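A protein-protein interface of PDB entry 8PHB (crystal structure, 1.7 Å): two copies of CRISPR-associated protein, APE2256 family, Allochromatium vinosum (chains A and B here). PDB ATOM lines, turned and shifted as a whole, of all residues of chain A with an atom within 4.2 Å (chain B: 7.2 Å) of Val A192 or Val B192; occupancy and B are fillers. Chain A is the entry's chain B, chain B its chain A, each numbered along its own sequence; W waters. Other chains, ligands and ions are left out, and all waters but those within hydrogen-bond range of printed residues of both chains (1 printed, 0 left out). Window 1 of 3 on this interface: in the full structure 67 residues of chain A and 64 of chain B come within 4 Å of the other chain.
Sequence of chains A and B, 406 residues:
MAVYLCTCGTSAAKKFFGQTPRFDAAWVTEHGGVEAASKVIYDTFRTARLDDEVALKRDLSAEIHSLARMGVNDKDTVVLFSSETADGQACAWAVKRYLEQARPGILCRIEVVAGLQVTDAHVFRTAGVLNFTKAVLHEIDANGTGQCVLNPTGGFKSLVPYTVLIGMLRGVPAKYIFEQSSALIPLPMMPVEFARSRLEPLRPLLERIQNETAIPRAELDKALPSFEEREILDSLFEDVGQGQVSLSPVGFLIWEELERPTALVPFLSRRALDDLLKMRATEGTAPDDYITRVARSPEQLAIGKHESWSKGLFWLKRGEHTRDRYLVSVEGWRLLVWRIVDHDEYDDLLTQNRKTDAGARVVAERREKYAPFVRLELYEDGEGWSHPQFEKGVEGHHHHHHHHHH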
ATOM      1  N   MET A 168      -2.553   9.076  18.979  1.00  0.00           N
ATOM      2  CA  MET A 168      -3.777   9.645  19.551  1.00  0.00           C
ATOM      3  C   MET A 168      -4.099   9.013  20.900  1.00  0.00           C
ATOM      4  O   MET A 168      -4.424   9.710  21.870  1.00  0.00           O
ATOM      5  CB  MET A 168      -4.951   9.448  18.583  1.00  0.00           C
ATOM      6  CG  MET A 168      -5.076  10.492  17.473  1.00  0.00           C
ATOM      7  SD  MET A 168      -6.263  10.008  16.185  1.00  0.00           S
ATOM      8  CE  MET A 168      -7.788  10.040  17.130  1.00  0.00           C
ATOM      9  N   MET A 190      -6.711  13.994  16.086  1.00  0.00           N
ATOM     10  CA  MET A 190      -7.985  14.627  16.394  1.00  0.00           C
ATOM     11  C   MET A 190      -8.399  14.278  17.809  1.00  0.00           C
ATOM     12  O   MET A 190      -8.401  13.093  18.169  1.00  0.00           O
ATOM     13  CB  MET A 190      -9.053  14.175  15.414  1.00  0.00           C
ATOM     14  CG  MET A 190     -10.443  14.572  15.794  1.00  0.00           C
ATOM     15  SD  MET A 190     -11.488  14.411  14.356  1.00  0.00           S
ATOM     16  CE  MET A 190     -13.114  14.698  15.068  1.00  0.00           C
ATOM     17  N   PRO A 191      -8.720  15.262  18.644  1.00  0.00           N
ATOM     18  CA  PRO A 191      -9.198  14.955  20.001  1.00  0.00           C
ATOM     19  C   PRO A 191     -10.540  14.245  19.925  1.00  0.00           C
ATOM     20  O   PRO A 191     -11.489  14.744  19.320  1.00  0.00           O
ATOM     21  CB  PRO A 191      -9.312  16.328  20.660  1.00  0.00           C
ATOM     22  CG  PRO A 191      -9.412  17.286  19.532  1.00  0.00           C
ATOM     23  CD  PRO A 191      -8.662  16.709  18.384  1.00  0.00           C
ATOM     24  N   VAL A 192     -10.599  13.053  20.518  1.00  0.00           N
ATOM     25  CA  VAL A 192     -11.802  12.231  20.546  1.00  0.00           C
ATOM     26  C   VAL A 192     -11.936  11.632  21.941  1.00  0.00           C
ATOM     27  O   VAL A 192     -10.997  11.639  22.741  1.00  0.00           O
ATOM     28  CB  VAL A 192     -11.769  11.111  19.486  1.00  0.00           C
ATOM     29  CG1 VAL A 192     -11.759  11.693  18.078  1.00  0.00           C
ATOM     30  CG2 VAL A 192     -10.547  10.227  19.699  1.00  0.00           C
ATOM     31  N   GLU A 193     -13.124  11.115  22.231  1.00  0.00           N
ATOM     32  CA  GLU A 193     -13.341  10.299  23.418  1.00  0.00           C
ATOM     33  C   GLU A 193     -13.455   8.837  23.005  1.00  0.00           C
ATOM     34  O   GLU A 193     -14.034   8.513  21.963  1.00  0.00           O
ATOM     35  CB  GLU A 193     -14.591  10.742  24.184  1.00  0.00           C
ATOM     36  N   ALA A 195     -14.999   5.372  22.705  1.00  0.00           N
ATOM     37  CA  ALA A 195     -16.430   5.043  22.630  1.00  0.00           C
ATOM     38  C   ALA A 195     -16.762   3.850  23.537  1.00  0.00           C
ATOM     39  O   ALA A 195     -17.163   2.774  23.092  1.00  0.00           O
ATOM     40  CB  ALA A 195     -16.820   4.756  21.187  1.00  0.00           C
ATOM     41  N   LEU B 165      -9.231  10.254   8.723  1.00  0.00           N
ATOM     42  CA  LEU B 165     -10.174  11.050   9.501  1.00  0.00           C
ATOM     43  C   LEU B 165     -11.467  11.313   8.738  1.00  0.00           C
ATOM     44  O   LEU B 165     -12.562  11.259   9.317  1.00  0.00           O
ATOM     45  CB  LEU B 165      -9.521  12.369   9.900  1.00  0.00           C
ATOM     46  CG  LEU B 165      -8.394  12.263  10.919  1.00  0.00           C
ATOM     47  CD1 LEU B 165      -7.702  13.610  11.053  1.00  0.00           C
ATOM     48  CD2 LEU B 165      -8.962  11.813  12.258  1.00  0.00           C
ATOM     49  N   MET B 168     -13.408   8.083   8.679  1.00  0.00           N
ATOM     50  CA  MET B 168     -13.991   7.845  10.001  1.00  0.00           C
ATOM     51  C   MET B 168     -15.209   8.732  10.248  1.00  0.00           C
ATOM     52  O   MET B 168     -16.243   8.261  10.740  1.00  0.00           O
ATOM     53  CB  MET B 168     -12.938   8.082  11.089  1.00  0.00           C
ATOM     54  CG  MET B 168     -12.162   6.837  11.527  1.00  0.00           C
ATOM     55  SD  MET B 168     -10.628   7.199  12.424  1.00  0.00           S
ATOM     56  CE  MET B 168     -11.261   8.195  13.782  1.00  0.00           C
ATOM     57  N   LEU B 169     -15.109  10.020   9.923  1.00  0.00           N
ATOM     58  CA  LEU B 169     -16.165  10.947  10.306  1.00  0.00           C
ATOM     59  C   LEU B 169     -17.401  10.821   9.426  1.00  0.00           C
ATOM     60  O   LEU B 169     -18.527  10.959   9.917  1.00  0.00           O
ATOM     61  CB  LEU B 169     -15.623  12.372  10.300  1.00  0.00           C
ATOM     62  CG  LEU B 169     -14.594  12.601  11.416  1.00  0.00           C
ATOM     63  CD1 LEU B 169     -14.093  14.048  11.424  1.00  0.00           C
ATOM     64  CD2 LEU B 169     -15.162  12.199  12.795  1.00  0.00           C
ATOM     65  N   MET B 189     -10.150   1.971  10.872  1.00  0.00           N
ATOM     66  CA  MET B 189     -11.161   2.919  11.330  1.00  0.00           C
ATOM     67  C   MET B 189     -11.405   2.628  12.805  1.00  0.00           C
ATOM     68  O   MET B 189     -11.881   1.550  13.154  1.00  0.00           O
ATOM     69  CB  MET B 189     -12.452   2.790  10.519  1.00  0.00           C
ATOM     70  CG  MET B 189     -12.282   3.056   9.020  1.00  0.00           C
ATOM     71  SD  MET B 189     -12.518   4.794   8.537  1.00  0.00           S
ATOM     72  CE  MET B 189     -10.927   5.207   7.832  1.00  0.00           C
ATOM     73  N   MET B 190     -11.038   3.559  13.673  1.00  0.00           N
ATOM     74  CA  MET B 190     -11.284   3.391  15.101  1.00  0.00           C
ATOM     75  C   MET B 190     -12.623   4.022  15.458  1.00  0.00           C
ATOM     76  O   MET B 190     -12.816   5.223  15.205  1.00  0.00           O
ATOM     77  CB  MET B 190     -10.164   4.027  15.908  1.00  0.00           C
ATOM     78  CG  MET B 190     -10.469   4.255  17.373  1.00  0.00           C
ATOM     79  SD  MET B 190     -10.270   2.794  18.401  1.00  0.00           S
ATOM     80  CE  MET B 190      -8.503   2.525  18.232  1.00  0.00           C
ATOM     81  N   PRO B 191     -13.585   3.264  15.991  1.00  0.00           N
ATOM     82  CA  PRO B 191     -14.824   3.887  16.483  1.00  0.00           C
ATOM     83  C   PRO B 191     -14.519   4.797  17.661  1.00  0.00           C
ATOM     84  O   PRO B 191     -13.978   4.357  18.676  1.00  0.00           O
ATOM     85  CB  PRO B 191     -15.695   2.696  16.893  1.00  0.00           C
ATOM     86  CG  PRO B 191     -14.736   1.520  17.029  1.00  0.00           C
ATOM     87  CD  PRO B 191     -13.630   1.789  16.057  1.00  0.00           C
ATOM     88  N   VAL B 192     -14.863   6.074  17.516  1.00  0.00           N
ATOM     89  CA  VAL B 192     -14.610   7.078  18.538  1.00  0.00           C
ATOM     90  C   VAL B 192     -15.882   7.883  18.775  1.00  0.00           C
ATOM     91  O   VAL B 192     -16.813   7.878  17.970  1.00  0.00           O
ATOM     92  CB  VAL B 192     -13.461   8.035  18.167  1.00  0.00           C
ATOM     93  CG1 VAL B 192     -12.146   7.282  18.089  1.00  0.00           C
ATOM     94  CG2 VAL B 192     -13.768   8.742  16.854  1.00  0.00           C
ATOM     95  N   GLU B 193     -15.888   8.585  19.899  1.00  0.00           N
ATOM     96  CA  GLU B 193     -16.930   9.535  20.251  1.00  0.00           C
ATOM     97  C   GLU B 193     -16.348  10.936  20.145  1.00  0.00           C
ATOM     98  O   GLU B 193     -15.217  11.181  20.581  1.00  0.00           O
ATOM     99  CB  GLU B 193     -17.465   9.273  21.665  1.00  0.00           C
ATOM    100  N   PHE B 194     -17.097  11.835  19.515  1.00  0.00           N
ATOM    101  CA  PHE B 194     -16.785  13.254  19.574  1.00  0.00           C
ATOM    102  C   PHE B 194     -16.661  13.700  21.027  1.00  0.00           C
ATOM    103  O   PHE B 194     -17.517  13.387  21.857  1.00  0.00           O
ATOM    104  CB  PHE B 194     -17.896  14.035  18.876  1.00  0.00           C
ATOM    105  CG  PHE B 194     -17.408  15.156  18.017  1.00  0.00           C
ATOM    106  CD1 PHE B 194     -16.960  14.908  16.734  1.00  0.00           C
ATOM    107  CD2 PHE B 194     -17.413  16.459  18.484  1.00  0.00           C
ATOM    108  CE1 PHE B 194     -16.515  15.934  15.933  1.00  0.00           C
ATOM    109  CE2 PHE B 194     -16.968  17.490  17.682  1.00  0.00           C
ATOM    110  CZ  PHE B 194     -16.521  17.222  16.406  1.00  0.00           C
ATOM    111  N   ALA B 195     -15.590  14.426  21.340  1.00  0.00           N
ATOM    112  CA  ALA B 195     -15.440  15.011  22.674  1.00  0.00           C
ATOM    113  C   ALA B 195     -16.278  16.291  22.775  1.00  0.00           C
ATOM    114  O   ALA B 195     -15.770  17.392  22.981  1.00  0.00           O
ATOM    115  CB  ALA B 195     -13.968  15.275  22.962  1.00  0.00           C
ATOM    116  N   LEU B 199     -15.271  20.084  23.596  1.00  0.00           N
ATOM    117  CA  LEU B 199     -15.125  20.942  22.426  1.00  0.00           C
ATOM    118  C   LEU B 199     -16.211  22.008  22.314  1.00  0.00           C
ATOM    119  O   LEU B 199     -15.942  23.089  21.781  1.00  0.00           O
ATOM    120  CB  LEU B 199     -15.102  20.087  21.154  1.00  0.00           C
ATOM    121  CG  LEU B 199     -13.887  19.153  21.034  1.00  0.00           C
ATOM    122  CD1 LEU B 199     -14.010  18.187  19.858  1.00  0.00           C
ATOM    123  CD2 LEU B 199     -12.616  19.953  20.905  1.00  0.00           C
ATOM    124  N   ILE B 254     -14.088  19.589  13.037  1.00  0.00           N
ATOM    125  CA  ILE B 254     -14.804  19.777  14.299  1.00  0.00           C
ATOM    126  C   ILE B 254     -15.777  20.946  14.189  1.00  0.00           C
ATOM    127  O   ILE B 254     -16.932  20.856  14.613  1.00  0.00           O
ATOM    128  CB  ILE B 254     -13.798  19.976  15.439  1.00  0.00           C
ATOM    129  CG1 ILE B 254     -13.135  18.635  15.783  1.00  0.00           C
ATOM    130  CG2 ILE B 254     -14.466  20.566  16.680  1.00  0.00           C
ATOM    131  CD1 ILE B 254     -11.866  18.768  16.609  1.00  0.00           C
HETATM  132  O   HOH W   1     -13.926  14.878  18.748  1.00  0.00           O
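The backbone NH (N) of Glu A193 is in hydrogen-bond range of the backbone carbonyl oxygen (O) of Glu B193 (2.7 Å).
CB of Met A190 touches CD2 of Leu B165, 3.9 Å away. CE of Met A190 touches CD1 of Leu B169, 3.8 Å away. Met A190 touches Phe B194. Val B192 touches Val A192. Val A192 touches Glu B193 (CA to O, 3.6 Å). Glu A193 touches Val B192. Ala A195 touches Pro B191.
Printed residues of chain B within 4 Å of Met A190: Leu B165 (3.9 Å), Leu B169 (3.8 Å) and Phe B194 (3.7 Å). Pro A191 touches none of the printed residues of chain B. Of the printed residues of chain A, Leu B165 touches Met A190 (3.9 Å). Met B189 touches none of the printed residues of chain A. Of the printed residues of chain A, Pro B191 touches Ala A195 (3.8 Å).
Of the 12 printed residues of chain B, 6 touch a printed residue of chain A. Hydrophobic or aromatic side chains of chain B that line the printed part of chain A: Leu B165, Leu B169, Val B192 and Phe B194. Printed residues of chain A that touch a printed residue of chain B: Met A190, Val A192, Glu A193 and Ala A195.
Val A192 touches its own counterpart, Val B192. Val A192 touches Glu B193, and with the chains exchanged Glu A193 touches Val B192. Glu A193 touches its own counterpart, Glu B193. Ala A195 touches Pro B191, but with the chains exchanged Pro A191 does not touch Ala B195 (4.4 Å). Of the 8 pairs that touch across the chains among the printed residues, 4 have their exchanged pair printed and touching as well.
Water W1 lies within hydrogen-bond range of O of Pro A191 and N of Ala B195.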
